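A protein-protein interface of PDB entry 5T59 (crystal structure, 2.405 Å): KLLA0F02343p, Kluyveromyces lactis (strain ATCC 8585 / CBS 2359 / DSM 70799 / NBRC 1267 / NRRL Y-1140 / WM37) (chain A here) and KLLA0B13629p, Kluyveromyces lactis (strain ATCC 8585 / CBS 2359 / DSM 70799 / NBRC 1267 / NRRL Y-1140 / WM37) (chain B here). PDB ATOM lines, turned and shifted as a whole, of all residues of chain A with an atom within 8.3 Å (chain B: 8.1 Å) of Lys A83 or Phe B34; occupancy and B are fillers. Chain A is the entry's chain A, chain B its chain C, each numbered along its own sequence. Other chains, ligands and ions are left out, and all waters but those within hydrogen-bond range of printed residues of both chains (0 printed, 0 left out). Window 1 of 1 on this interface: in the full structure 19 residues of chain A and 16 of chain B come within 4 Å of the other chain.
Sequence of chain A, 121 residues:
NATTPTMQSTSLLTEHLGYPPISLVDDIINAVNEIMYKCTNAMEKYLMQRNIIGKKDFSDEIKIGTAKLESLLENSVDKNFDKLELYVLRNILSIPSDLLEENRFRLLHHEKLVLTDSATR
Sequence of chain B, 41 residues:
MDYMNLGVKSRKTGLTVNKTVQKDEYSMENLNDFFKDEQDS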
ATOM      1  N   VAL A  25       7.283 -20.304  13.040  1.00  0.00           N
ATOM      2  CA  VAL A  25       7.401 -18.929  12.571  1.00  0.00           C
ATOM      3  C   VAL A  25       8.246 -18.109  13.539  1.00  0.00           C
ATOM      4  O   VAL A  25       9.036 -17.253  13.123  1.00  0.00           O
ATOM      5  CB  VAL A  25       6.002 -18.317  12.375  1.00  0.00           C
ATOM      6  CG1 VAL A  25       6.104 -16.856  11.961  1.00  0.00           C
ATOM      7  CG2 VAL A  25       5.212 -19.112  11.348  1.00  0.00           C
ATOM      8  N   ILE A  29      11.491 -15.820  12.347  1.00  0.00           N
ATOM      9  CA  ILE A  29      11.586 -14.382  12.583  1.00  0.00           C
ATOM     10  C   ILE A  29      12.723 -14.091  13.551  1.00  0.00           C
ATOM     11  O   ILE A  29      13.594 -13.256  13.287  1.00  0.00           O
ATOM     12  CB  ILE A  29      10.245 -13.838  13.108  1.00  0.00           C
ATOM     13  CG1 ILE A  29       9.159 -14.010  12.051  1.00  0.00           C
ATOM     14  CG2 ILE A  29      10.373 -12.360  13.483  1.00  0.00           C
ATOM     15  CD1 ILE A  29       7.761 -13.731  12.552  1.00  0.00           C
ATOM     16  N   SER A  76      11.873  -3.466   6.353  1.00  0.00           N
ATOM     17  CA  SER A  76      11.640  -4.386   5.243  1.00  0.00           C
ATOM     18  C   SER A  76      11.504  -5.824   5.731  1.00  0.00           C
ATOM     19  O   SER A  76      10.650  -6.573   5.242  1.00  0.00           O
ATOM     20  CB  SER A  76      12.775  -4.266   4.225  1.00  0.00           C
ATOM     21  OG  SER A  76      12.600  -5.163   3.140  1.00  0.00           O
ATOM     22  N   VAL A  77      12.334  -6.226   6.695  1.00  0.00           N
ATOM     23  CA  VAL A  77      12.249  -7.576   7.246  1.00  0.00           C
ATOM     24  C   VAL A  77      10.937  -7.767   7.994  1.00  0.00           C
ATOM     25  O   VAL A  77      10.185  -8.714   7.730  1.00  0.00           O
ATOM     26  CB  VAL A  77      13.469  -7.851   8.142  1.00  0.00           C
ATOM     27  CG1 VAL A  77      13.307  -9.138   8.943  1.00  0.00           C
ATOM     28  CG2 VAL A  77      14.708  -7.947   7.260  1.00  0.00           C
ATOM     29  N   ASP A  78      10.640  -6.871   8.936  1.00  0.00           N
ATOM     30  CA  ASP A  78       9.364  -6.951   9.630  1.00  0.00           C
ATOM     31  C   ASP A  78       8.221  -7.003   8.634  1.00  0.00           C
ATOM     32  O   ASP A  78       7.235  -7.716   8.851  1.00  0.00           O
ATOM     33  CB  ASP A  78       9.205  -5.755  10.571  1.00  0.00           C
ATOM     34  CG  ASP A  78      10.157  -5.812  11.754  1.00  0.00           C
ATOM     35  OD1 ASP A  78      10.716  -6.900  12.018  1.00  0.00           O
ATOM     36  OD2 ASP A  78      10.357  -4.768  12.414  1.00  0.00           O
ATOM     37  N   LYS A  79       8.361  -6.301   7.511  1.00  0.00           N
ATOM     38  CA  LYS A  79       7.317  -6.296   6.493  1.00  0.00           C
ATOM     39  C   LYS A  79       7.224  -7.645   5.794  1.00  0.00           C
ATOM     40  O   LYS A  79       6.145  -8.241   5.716  1.00  0.00           O
ATOM     41  CB  LYS A  79       7.591  -5.185   5.479  1.00  0.00           C
ATOM     42  CG  LYS A  79       6.555  -5.065   4.365  1.00  0.00           C
ATOM     43  CD  LYS A  79       6.902  -3.909   3.436  1.00  0.00           C
ATOM     44  CE  LYS A  79       5.908  -3.776   2.300  1.00  0.00           C
ATOM     45  NZ  LYS A  79       6.248  -2.640   1.396  1.00  0.00           N
ATOM     46  N   ASN A  80       8.348  -8.142   5.275  1.00  0.00           N
ATOM     47  CA  ASN A  80       8.322  -9.321   4.418  1.00  0.00           C
ATOM     48  C   ASN A  80       8.097 -10.609   5.198  1.00  0.00           C
ATOM     49  O   ASN A  80       7.577 -11.578   4.634  1.00  0.00           O
ATOM     50  CB  ASN A  80       9.626  -9.426   3.634  1.00  0.00           C
ATOM     51  CG  ASN A  80       9.743  -8.378   2.561  1.00  0.00           C
ATOM     52  OD1 ASN A  80       9.142  -8.501   1.493  1.00  0.00           O
ATOM     53  ND2 ASN A  80      10.514  -7.336   2.833  1.00  0.00           N
ATOM     54  N   PHE A  81       8.501 -10.654   6.467  1.00  0.00           N
ATOM     55  CA  PHE A  81       8.310 -11.846   7.283  1.00  0.00           C
ATOM     56  C   PHE A  81       6.976 -11.883   8.015  1.00  0.00           C
ATOM     57  O   PHE A  81       6.593 -12.950   8.505  1.00  0.00           O
ATOM     58  CB  PHE A  81       9.465 -11.993   8.278  1.00  0.00           C
ATOM     59  CG  PHE A  81      10.741 -12.491   7.645  1.00  0.00           C
ATOM     60  CD1 PHE A  81      10.985 -13.855   7.520  1.00  0.00           C
ATOM     61  CD2 PHE A  81      11.666 -11.606   7.130  1.00  0.00           C
ATOM     62  CE1 PHE A  81      12.142 -14.318   6.926  1.00  0.00           C
ATOM     63  CE2 PHE A  81      12.829 -12.067   6.532  1.00  0.00           C
ATOM     64  CZ  PHE A  81      13.065 -13.423   6.427  1.00  0.00           C
ATOM     65  N   ASP A  82       6.247 -10.767   8.101  1.00  0.00           N
ATOM     66  CA  ASP A  82       4.855 -10.863   8.528  1.00  0.00           C
ATOM     67  C   ASP A  82       3.986 -11.462   7.427  1.00  0.00           C
ATOM     68  O   ASP A  82       3.098 -12.273   7.707  1.00  0.00           O
ATOM     69  CB  ASP A  82       4.325  -9.498   8.968  1.00  0.00           C
ATOM     70  CG  ASP A  82       4.805  -9.104  10.358  1.00  0.00           C
ATOM     71  OD1 ASP A  82       5.276  -9.994  11.094  1.00  0.00           O
ATOM     72  OD2 ASP A  82       4.673  -7.917  10.733  1.00  0.00           O
ATOM     73  N   LYS A  83       4.240 -11.099   6.167  1.00  0.00           N
ATOM     74  CA  LYS A  83       3.586 -11.795   5.062  1.00  0.00           C
ATOM     75  C   LYS A  83       3.875 -13.291   5.117  1.00  0.00           C
ATOM     76  O   LYS A  83       2.973 -14.115   4.913  1.00  0.00           O
ATOM     77  CB  LYS A  83       4.043 -11.216   3.723  1.00  0.00           C
ATOM     78  CG  LYS A  83       3.613  -9.780   3.463  1.00  0.00           C
ATOM     79  CD  LYS A  83       4.162  -9.275   2.134  1.00  0.00           C
ATOM     80  CE  LYS A  83       3.721  -7.852   1.846  1.00  0.00           C
ATOM     81  NZ  LYS A  83       4.290  -7.336   0.572  1.00  0.00           N
ATOM     82  N   LEU A  84       5.127 -13.661   5.394  1.00  0.00           N
ATOM     83  CA  LEU A  84       5.464 -15.059   5.636  1.00  0.00           C
ATOM     84  C   LEU A  84       4.593 -15.637   6.745  1.00  0.00           C
ATOM     85  O   LEU A  84       3.901 -16.644   6.554  1.00  0.00           O
ATOM     86  CB  LEU A  84       6.946 -15.168   6.001  1.00  0.00           C
ATOM     87  CG  LEU A  84       7.458 -16.549   6.415  1.00  0.00           C
ATOM     88  CD1 LEU A  84       7.380 -17.528   5.265  1.00  0.00           C
ATOM     89  CD2 LEU A  84       8.879 -16.444   6.936  1.00  0.00           C
ATOM     90  N   GLU A  85       4.603 -14.990   7.916  1.00  0.00           N
ATOM     91  CA  GLU A  85       3.771 -15.437   9.031  1.00  0.00           C
ATOM     92  C   GLU A  85       2.346 -15.694   8.572  1.00  0.00           C
ATOM     93  O   GLU A  85       1.687 -16.624   9.051  1.00  0.00           O
ATOM     94  CB  GLU A  85       3.798 -14.395  10.156  1.00  0.00           C
ATOM     95  CG  GLU A  85       2.965 -14.758  11.373  1.00  0.00           C
ATOM     96  CD  GLU A  85       3.075 -13.724  12.482  1.00  0.00           C
ATOM     97  OE1 GLU A  85       3.778 -12.710  12.283  1.00  0.00           O
ATOM     98  OE2 GLU A  85       2.459 -13.922  13.550  1.00  0.00           O
ATOM     99  N   LEU A  86       1.863 -14.891   7.628  1.00  0.00           N
ATOM    100  CA  LEU A  86       0.503 -15.045   7.129  1.00  0.00           C
ATOM    101  C   LEU A  86       0.430 -16.096   6.030  1.00  0.00           C
ATOM    102  O   LEU A  86      -0.442 -16.972   6.058  1.00  0.00           O
ATOM    103  CB  LEU A  86      -0.021 -13.695   6.631  1.00  0.00           C
ATOM    104  CG  LEU A  86      -0.725 -12.827   7.682  1.00  0.00           C
ATOM    105  CD1 LEU A  86       0.171 -12.495   8.864  1.00  0.00           C
ATOM    106  CD2 LEU A  86      -1.192 -11.553   7.031  1.00  0.00           C
ATOM    107  N   TYR A  87       1.346 -16.047   5.062  1.00  0.00           N
ATOM    108  CA  TYR A  87       1.263 -16.994   3.960  1.00  0.00           C
ATOM    109  C   TYR A  87       1.394 -18.428   4.451  1.00  0.00           C
ATOM    110  O   TYR A  87       0.798 -19.342   3.868  1.00  0.00           O
ATOM    111  CB  TYR A  87       2.342 -16.718   2.920  1.00  0.00           C
ATOM    112  CG  TYR A  87       2.175 -17.590   1.703  1.00  0.00           C
ATOM    113  CD1 TYR A  87       1.339 -17.206   0.666  1.00  0.00           C
ATOM    114  CD2 TYR A  87       2.793 -18.829   1.619  1.00  0.00           C
ATOM    115  CE1 TYR A  87       1.161 -18.007  -0.441  1.00  0.00           C
ATOM    116  CE2 TYR A  87       2.616 -19.642   0.519  1.00  0.00           C
ATOM    117  CZ  TYR A  87       1.799 -19.226  -0.508  1.00  0.00           C
ATOM    118  OH  TYR A  87       1.627 -20.037  -1.604  1.00  0.00           O
ATOM    119  N   VAL A  88       2.181 -18.650   5.507  1.00  0.00           N
ATOM    120  CA  VAL A  88       2.386 -20.004   6.015  1.00  0.00           C
ATOM    121  C   VAL A  88       1.133 -20.501   6.720  1.00  0.00           C
ATOM    122  O   VAL A  88       0.583 -21.558   6.383  1.00  0.00           O
ATOM    123  CB  VAL A  88       3.608 -20.044   6.950  1.00  0.00           C
ATOM    124  CG1 VAL A  88       3.765 -21.433   7.584  1.00  0.00           C
ATOM    125  CG2 VAL A  88       4.869 -19.656   6.192  1.00  0.00           C
ATOM    126  N   LEU A  89       0.657 -19.744   7.708  1.00  0.00           N
ATOM    127  CA  LEU A  89      -0.478 -20.178   8.509  1.00  0.00           C
ATOM    128  C   LEU A  89      -1.744 -20.345   7.683  1.00  0.00           C
ATOM    129  O   LEU A  89      -2.690 -20.986   8.156  1.00  0.00           O
ATOM    130  CB  LEU A  89      -0.711 -19.175   9.639  1.00  0.00           C
ATOM    131  CG  LEU A  89       0.446 -19.031  10.636  1.00  0.00           C
ATOM    132  CD1 LEU A  89       0.169 -17.911  11.628  1.00  0.00           C
ATOM    133  CD2 LEU A  89       0.718 -20.334  11.376  1.00  0.00           C
ATOM    134  N   ARG A  90      -1.777 -19.817   6.458  1.00  0.00           N
ATOM    135  CA  ARG A  90      -2.964 -19.862   5.615  1.00  0.00           C
ATOM    136  C   ARG A  90      -2.874 -20.876   4.484  1.00  0.00           C
ATOM    137  O   ARG A  90      -3.907 -21.405   4.070  1.00  0.00           O
ATOM    138  CB  ARG A  90      -3.237 -18.473   5.019  1.00  0.00           C
ATOM    139  CG  ARG A  90      -3.455 -17.385   6.080  1.00  0.00           C
ATOM    140  CD  ARG A  90      -3.632 -15.992   5.480  1.00  0.00           C
ATOM    141  NE  ARG A  90      -4.812 -15.904   4.615  1.00  0.00           N
ATOM    142  CZ  ARG A  90      -4.793 -15.749   3.294  1.00  0.00           C
ATOM    143  NH1 ARG A  90      -3.649 -15.664   2.624  1.00  0.00           N
ATOM    144  NH2 ARG A  90      -5.938 -15.679   2.626  1.00  0.00           N
ATOM    145  N   ASN A  91      -1.672 -21.184   3.993  1.00  0.00           N
ATOM    146  CA  ASN A  91      -1.493 -22.058   2.838  1.00  0.00           C
ATOM    147  C   ASN A  91      -0.667 -23.295   3.129  1.00  0.00           C
ATOM    148  O   ASN A  91      -0.882 -24.325   2.489  1.00  0.00           O
ATOM    149  CB  ASN A  91      -0.815 -21.298   1.693  1.00  0.00           C
ATOM    150  CG  ASN A  91      -1.653 -20.168   1.180  1.00  0.00           C
ATOM    151  OD1 ASN A  91      -2.665 -20.385   0.515  1.00  0.00           O
ATOM    152  ND2 ASN A  91      -1.237 -18.944   1.485  1.00  0.00           N
ATOM    153  N   GLY B   7      -5.274 -15.207  11.385  1.00  0.00           N
ATOM    154  CA  GLY B   7      -5.765 -15.325  10.027  1.00  0.00           C
ATOM    155  C   GLY B   7      -5.361 -14.188   9.116  1.00  0.00           C
ATOM    156  O   GLY B   7      -5.020 -14.408   7.950  1.00  0.00           O
ATOM    157  N   SER B  10      -1.048  -9.790  11.379  1.00  0.00           N
ATOM    158  CA  SER B  10       0.352 -10.029  11.700  1.00  0.00           C
ATOM    159  C   SER B  10       0.635  -9.528  13.110  1.00  0.00           C
ATOM    160  O   SER B  10       0.315  -8.385  13.448  1.00  0.00           O
ATOM    161  CB  SER B  10       1.254  -9.319  10.697  1.00  0.00           C
ATOM    162  OG  SER B  10       1.043  -9.816   9.390  1.00  0.00           O
ATOM    163  N   THR B  13       2.616  -6.157  13.081  1.00  0.00           N
ATOM    164  CA  THR B  13       2.279  -5.097  12.132  1.00  0.00           C
ATOM    165  C   THR B  13       0.851  -5.148  11.623  1.00  0.00           C
ATOM    166  O   THR B  13       0.360  -4.128  11.129  1.00  0.00           O
ATOM    167  CB  THR B  13       3.226  -5.139  10.926  1.00  0.00           C
ATOM    168  OG1 THR B  13       4.570  -4.936  11.373  1.00  0.00           O
ATOM    169  CG2 THR B  13       2.862  -4.062   9.893  1.00  0.00           C
ATOM    170  N   LEU B  15      -0.890  -6.955   8.941  1.00  0.00           N
ATOM    171  CA  LEU B  15      -1.008  -6.822   7.493  1.00  0.00           C
ATOM    172  C   LEU B  15      -2.181  -7.684   7.044  1.00  0.00           C
ATOM    173  O   LEU B  15      -2.035  -8.890   6.837  1.00  0.00           O
ATOM    174  CB  LEU B  15       0.288  -7.241   6.808  1.00  0.00           C
ATOM    175  CG  LEU B  15       1.527  -6.389   7.095  1.00  0.00           C
ATOM    176  CD1 LEU B  15       2.752  -7.024   6.468  1.00  0.00           C
ATOM    177  CD2 LEU B  15       1.344  -4.975   6.579  1.00  0.00           C
ATOM    178  N   THR B  16      -3.348  -7.070   6.889  1.00  0.00           N
ATOM    179  CA  THR B  16      -4.515  -7.813   6.432  1.00  0.00           C
ATOM    180  C   THR B  16      -4.327  -8.252   4.986  1.00  0.00           C
ATOM    181  O   THR B  16      -3.916  -7.459   4.133  1.00  0.00           O
ATOM    182  CB  THR B  16      -5.771  -6.953   6.560  1.00  0.00           C
ATOM    183  OG1 THR B  16      -5.951  -6.576   7.930  1.00  0.00           O
ATOM    184  CG2 THR B  16      -7.006  -7.715   6.076  1.00  0.00           C
ATOM    185  N   VAL B  17      -4.624  -9.523   4.711  1.00  0.00           N
ATOM    186  CA  VAL B  17      -4.542 -10.054   3.354  1.00  0.00           C
ATOM    187  C   VAL B  17      -5.771  -9.592   2.580  1.00  0.00           C
ATOM    188  O   VAL B  17      -6.575 -10.403   2.108  1.00  0.00           O
ATOM    189  CB  VAL B  17      -4.405 -11.593   3.358  1.00  0.00           C
ATOM    190  CG1 VAL B  17      -5.597 -12.269   4.047  1.00  0.00           C
ATOM    191  CG2 VAL B  17      -4.209 -12.127   1.938  1.00  0.00           C
ATOM    192  N   ASN B  18      -5.915  -8.276   2.437  1.00  0.00           N
ATOM    193  CA  ASN B  18      -7.071  -7.666   1.795  1.00  0.00           C
ATOM    194  C   ASN B  18      -6.973  -7.648   0.270  1.00  0.00           C
ATOM    195  O   ASN B  18      -7.688  -6.860  -0.363  1.00  0.00           O
ATOM    196  CB  ASN B  18      -7.259  -6.242   2.323  1.00  0.00           C
ATOM    197  CG  ASN B  18      -6.082  -5.340   2.000  1.00  0.00           C
ATOM    198  OD1 ASN B  18      -5.006  -5.811   1.631  1.00  0.00           O
ATOM    199  ND2 ASN B  18      -6.282  -4.037   2.138  1.00  0.00           N
ATOM    200  N   LYS B  19      -6.123  -8.474  -0.337  1.00  0.00           N
ATOM    201  CA  LYS B  19      -5.937  -8.462  -1.791  1.00  0.00           C
ATOM    202  C   LYS B  19      -6.979  -9.342  -2.484  1.00  0.00           C
ATOM    203  O   LYS B  19      -6.679 -10.152  -3.361  1.00  0.00           O
ATOM    204  CB  LYS B  19      -4.512  -8.895  -2.134  1.00  0.00           C
ATOM    205  CG  LYS B  19      -4.115  -8.753  -3.603  1.00  0.00           C
ATOM    206  CD  LYS B  19      -4.183  -7.297  -4.058  1.00  0.00           C
ATOM    207  CE  LYS B  19      -3.416  -7.075  -5.352  1.00  0.00           C
ATOM    208  NZ  LYS B  19      -3.948  -7.904  -6.466  1.00  0.00           N
ATOM    209  N   GLN B  22      -6.819 -12.970  -4.231  1.00  0.00           N
ATOM    210  CA  GLN B  22      -5.437 -13.413  -4.312  1.00  0.00           C
ATOM    211  C   GLN B  22      -5.202 -13.989  -5.707  1.00  0.00           C
ATOM    212  O   GLN B  22      -5.398 -13.289  -6.706  1.00  0.00           O
ATOM    213  CB  GLN B  22      -5.137 -14.437  -3.212  1.00  0.00           C
ATOM    214  CG  GLN B  22      -5.562 -13.983  -1.814  1.00  0.00           C
ATOM    215  CD  GLN B  22      -4.932 -12.680  -1.385  1.00  0.00           C
ATOM    216  OE1 GLN B  22      -5.587 -11.640  -1.384  1.00  0.00           O
ATOM    217  NE2 GLN B  22      -3.651 -12.724  -1.027  1.00  0.00           N
ATOM    218  N   LYS B  23      -4.792 -15.253  -5.796  1.00  0.00           N
ATOM    219  CA  LYS B  23      -4.723 -15.947  -7.078  1.00  0.00           C
ATOM    220  C   LYS B  23      -4.381 -17.412  -6.842  1.00  0.00           C
ATOM    221  O   LYS B  23      -3.233 -17.746  -6.541  1.00  0.00           O
ATOM    222  CB  LYS B  23      -3.688 -15.303  -8.004  1.00  0.00           C
ATOM    223  CG  LYS B  23      -3.636 -15.947  -9.380  1.00  0.00           C
ATOM    224  CD  LYS B  23      -2.717 -15.193 -10.324  1.00  0.00           C
ATOM    225  CE  LYS B  23      -2.646 -15.882 -11.676  1.00  0.00           C
ATOM    226  NZ  LYS B  23      -1.921 -17.185 -11.608  1.00  0.00           N
ATOM    227  N   GLU B  29      -2.548 -20.419  -3.158  1.00  0.00           N
ATOM    228  CA  GLU B  29      -2.452 -19.070  -3.698  1.00  0.00           C
ATOM    229  C   GLU B  29      -0.988 -18.714  -3.922  1.00  0.00           C
ATOM    230  O   GLU B  29      -0.136 -18.970  -3.067  1.00  0.00           O
ATOM    231  CB  GLU B  29      -3.108 -18.077  -2.741  1.00  0.00           C
ATOM    232  CG  GLU B  29      -2.434 -18.015  -1.389  1.00  0.00           C
ATOM    233  CD  GLU B  29      -3.236 -17.228  -0.371  1.00  0.00           C
ATOM    234  OE1 GLU B  29      -4.140 -16.472  -0.773  1.00  0.00           O
ATOM    235  OE2 GLU B  29      -2.966 -17.372   0.839  1.00  0.00           O
ATOM    236  N   ASN B  30      -0.699 -18.108  -5.074  1.00  0.00           N
ATOM    237  CA  ASN B  30       0.682 -17.981  -5.513  1.00  0.00           C
ATOM    238  C   ASN B  30       1.381 -16.848  -4.774  1.00  0.00           C
ATOM    239  O   ASN B  30       0.778 -15.822  -4.441  1.00  0.00           O
ATOM    240  CB  ASN B  30       0.774 -17.782  -7.031  1.00  0.00           C
ATOM    241  CG  ASN B  30       0.311 -16.414  -7.490  1.00  0.00           C
ATOM    242  OD1 ASN B  30      -0.336 -15.671  -6.754  1.00  0.00           O
ATOM    243  ND2 ASN B  30       0.661 -16.072  -8.726  1.00  0.00           N
ATOM    244  N   LEU B  31       2.667 -17.063  -4.500  1.00  0.00           N
ATOM    245  CA  LEU B  31       3.458 -16.099  -3.744  1.00  0.00           C
ATOM    246  C   LEU B  31       3.550 -14.767  -4.471  1.00  0.00           C
ATOM    247  O   LEU B  31       3.243 -13.714  -3.901  1.00  0.00           O
ATOM    248  CB  LEU B  31       4.853 -16.677  -3.516  1.00  0.00           C
ATOM    249  CG  LEU B  31       4.915 -17.916  -2.625  1.00  0.00           C
ATOM    250  CD1 LEU B  31       6.285 -18.559  -2.707  1.00  0.00           C
ATOM    251  CD2 LEU B  31       4.610 -17.535  -1.196  1.00  0.00           C
ATOM    252  N   ASN B  32       3.977 -14.796  -5.737  1.00  0.00           N
ATOM    253  CA  ASN B  32       4.260 -13.582  -6.491  1.00  0.00           C
ATOM    254  C   ASN B  32       3.258 -12.469  -6.200  1.00  0.00           C
ATOM    255  O   ASN B  32       3.631 -11.383  -5.742  1.00  0.00           O
ATOM    256  CB  ASN B  32       4.274 -13.915  -7.983  1.00  0.00           C
ATOM    257  CG  ASN B  32       5.431 -14.809  -8.359  1.00  0.00           C
ATOM    258  OD1 ASN B  32       6.569 -14.357  -8.471  1.00  0.00           O
ATOM    259  ND2 ASN B  32       5.149 -16.091  -8.543  1.00  0.00           N
ATOM    260  N   ASP B  33       1.973 -12.739  -6.424  1.00  0.00           N
ATOM    261  CA  ASP B  33       0.960 -11.727  -6.152  1.00  0.00           C
ATOM    262  C   ASP B  33       0.827 -11.463  -4.658  1.00  0.00           C
ATOM    263  O   ASP B  33       0.588 -10.320  -4.250  1.00  0.00           O
ATOM    264  CB  ASP B  33      -0.381 -12.169  -6.743  1.00  0.00           C
ATOM    265  CG  ASP B  33      -1.461 -11.103  -6.621  1.00  0.00           C
ATOM    266  OD1 ASP B  33      -1.185 -10.017  -6.068  1.00  0.00           O
ATOM    267  OD2 ASP B  33      -2.593 -11.353  -7.088  1.00  0.00           O
ATOM    268  N   PHE B  34       1.009 -12.496  -3.833  1.00  0.00           N
ATOM    269  CA  PHE B  34       0.776 -12.353  -2.400  1.00  0.00           C
ATOM    270  C   PHE B  34       1.740 -11.351  -1.775  1.00  0.00           C
ATOM    271  O   PHE B  34       1.365 -10.602  -0.865  1.00  0.00           O
ATOM    272  CB  PHE B  34       0.906 -13.713  -1.715  1.00  0.00           C
ATOM    273  CG  PHE B  34       0.530 -13.692  -0.262  1.00  0.00           C
ATOM    274  CD1 PHE B  34      -0.793 -13.847   0.118  1.00  0.00           C
ATOM    275  CD2 PHE B  34       1.486 -13.494   0.718  1.00  0.00           C
ATOM    276  CE1 PHE B  34      -1.156 -13.823   1.452  1.00  0.00           C
ATOM    277  CE2 PHE B  34       1.130 -13.464   2.056  1.00  0.00           C
ATOM    278  CZ  PHE B  34      -0.195 -13.629   2.423  1.00  0.00           C
ATOM    279  N   PHE B  35       2.983 -11.319  -2.252  1.00  0.00           N
ATOM    280  CA  PHE B  35       4.037 -10.473  -1.689  1.00  0.00           C
ATOM    281  C   PHE B  35       4.214  -9.161  -2.448  1.00  0.00           C
ATOM    282  O   PHE B  35       5.344  -8.733  -2.697  1.00  0.00           O
ATOM    283  CB  PHE B  35       5.356 -11.249  -1.645  1.00  0.00           C
ATOM    284  CG  PHE B  35       5.436 -12.252  -0.526  1.00  0.00           C
ATOM    285  CD1 PHE B  35       5.938 -11.876   0.713  1.00  0.00           C
ATOM    286  CD2 PHE B  35       4.997 -13.556  -0.697  1.00  0.00           C
ATOM    287  CE1 PHE B  35       6.018 -12.784   1.753  1.00  0.00           C
ATOM    288  CE2 PHE B  35       5.071 -14.465   0.343  1.00  0.00           C
ATOM    289  CZ  PHE B  35       5.580 -14.078   1.571  1.00  0.00           C
ATOM    290  N   LYS B  36       3.129  -8.483  -2.817  1.00  0.00           N
ATOM    291  CA  LYS B  36       3.260  -7.148  -3.396  1.00  0.00           C
ATOM    292  C   LYS B  36       2.011  -6.318  -3.147  1.00  0.00           C
ATOM    293  O   LYS B  36       0.896  -6.782  -3.381  1.00  0.00           O
ATOM    294  CB  LYS B  36       3.539  -7.237  -4.898  1.00  0.00           C
ATOM    295  CG  LYS B  36       3.907  -5.903  -5.527  1.00  0.00           C
ATOM    296  CD  LYS B  36       4.327  -6.062  -6.981  1.00  0.00           C
ATOM    297  CE  LYS B  36       4.745  -4.731  -7.585  1.00  0.00           C
ATOM    298  NZ  LYS B  36       5.195  -4.866  -8.999  1.00  0.00           N
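Lys A83 touches just these residues of chain B: Phe B34, Phe B35 and Lys B36. Of the printed residues of chain A, Phe B34 touches Lys A83 (3.5 Å), Tyr A87 (3.6 Å) and Arg A90 (3.3 Å). Phe B35 touches just these residues of chain A: Asn A80 (3.5 Å), Lys A83 (3.2 Å) and Leu A84 (3.8 Å). Printed residues of chain A within 4 Å of Glu B29: Tyr A87 (2.5 Å), Arg A90 (2.6 Å) and Asn A91 (2.4 Å). Of the printed residues of chain B, Lys A79 touches Leu B15. Of the printed residues of chain B, Leu A86 touches Ser B10 (2.9 Å) and Leu B15 (2.8 Å). Asn B30 touches none of the printed residues of chain A. The nearest residue of chain B that does not touch Lys A83 is Leu B15 (4.2 Å). The nearest printed residue of chain A that does not touch Ser B10 is Glu A85 (4.4 Å).
Hydrophobic or aromatic side chains of chain A within 4 Å of the printed part of chain B: Leu A86 and Tyr A87. Printed residues of chain B that touch a printed residue of chain A: Gly B7, Ser B10, Thr B13, Leu B15, Val B17, Glu B29, Leu B31, Phe B34, Phe B35 and Lys B36. Hydrophobic or aromatic side chains of chain B within 4 Å of the printed part of chain A: Leu B15, Val B17, Leu B31, Phe B34 and Phe B35. Among the printed residues, Asp or Glu carboxylates within 4 Å of a Lys or Arg side-chain nitrogen of the other chain: Arg A90 with Glu B29 (2.6 Å).
ND2 of Asn A91 is in hydrogen-bond range of OE2 of Glu B29, 2.4 Å away. OE2 of Glu B29 is in salt-bridge range of NH1 of Arg A90, at 2.6 Å. The side-chain hydroxyl (OH) of Tyr A87 is in hydrogen-bond range of the backbone carbonyl oxygen (O) of Glu B29 (2.5 Å). OD2 of Asp A82 sits at hydrogen-bond distance from OG1 of Thr B13 (3.1 Å).
Lys A79 touches Leu B15 (O to CD1, 3.7 Å). Phe B35 touches Asn A80 (CE1 to O, 3.5 Å). CD1 of Leu B15 touches CB of Asp A82, at 3.9 Å. NZ of Lys A83 touches N of Lys B36, 3.8 Å away. Ser B10 touches Leu A86 (OG to CD1, 2.9 Å). Leu A86 touches Leu B15 (CD2 to O, 2.8 Å). CE2 of Phe B34 touches CB of Tyr A87, 3.6 Å away. O of Gly B7 touches CD of Arg A90, 3.2 Å away. Arg A90 touches Val B17 (NH1 to CG2, 3.6 Å). Phe B34 touches Arg A90 (CE1 to NH1, 3.3 Å).
O of Ser A76 sits at hydrogen-bond distance from ND2 of Asn A80 (2.5 Å). The backbone carbonyl oxygen (O) of Tyr A87 is in hydrogen-bond range of the side-chain amide nitrogen (ND2) of Asn A91. OG of Ser B10 is in hydrogen-bond range of N of Leu B15 (3.5 Å).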
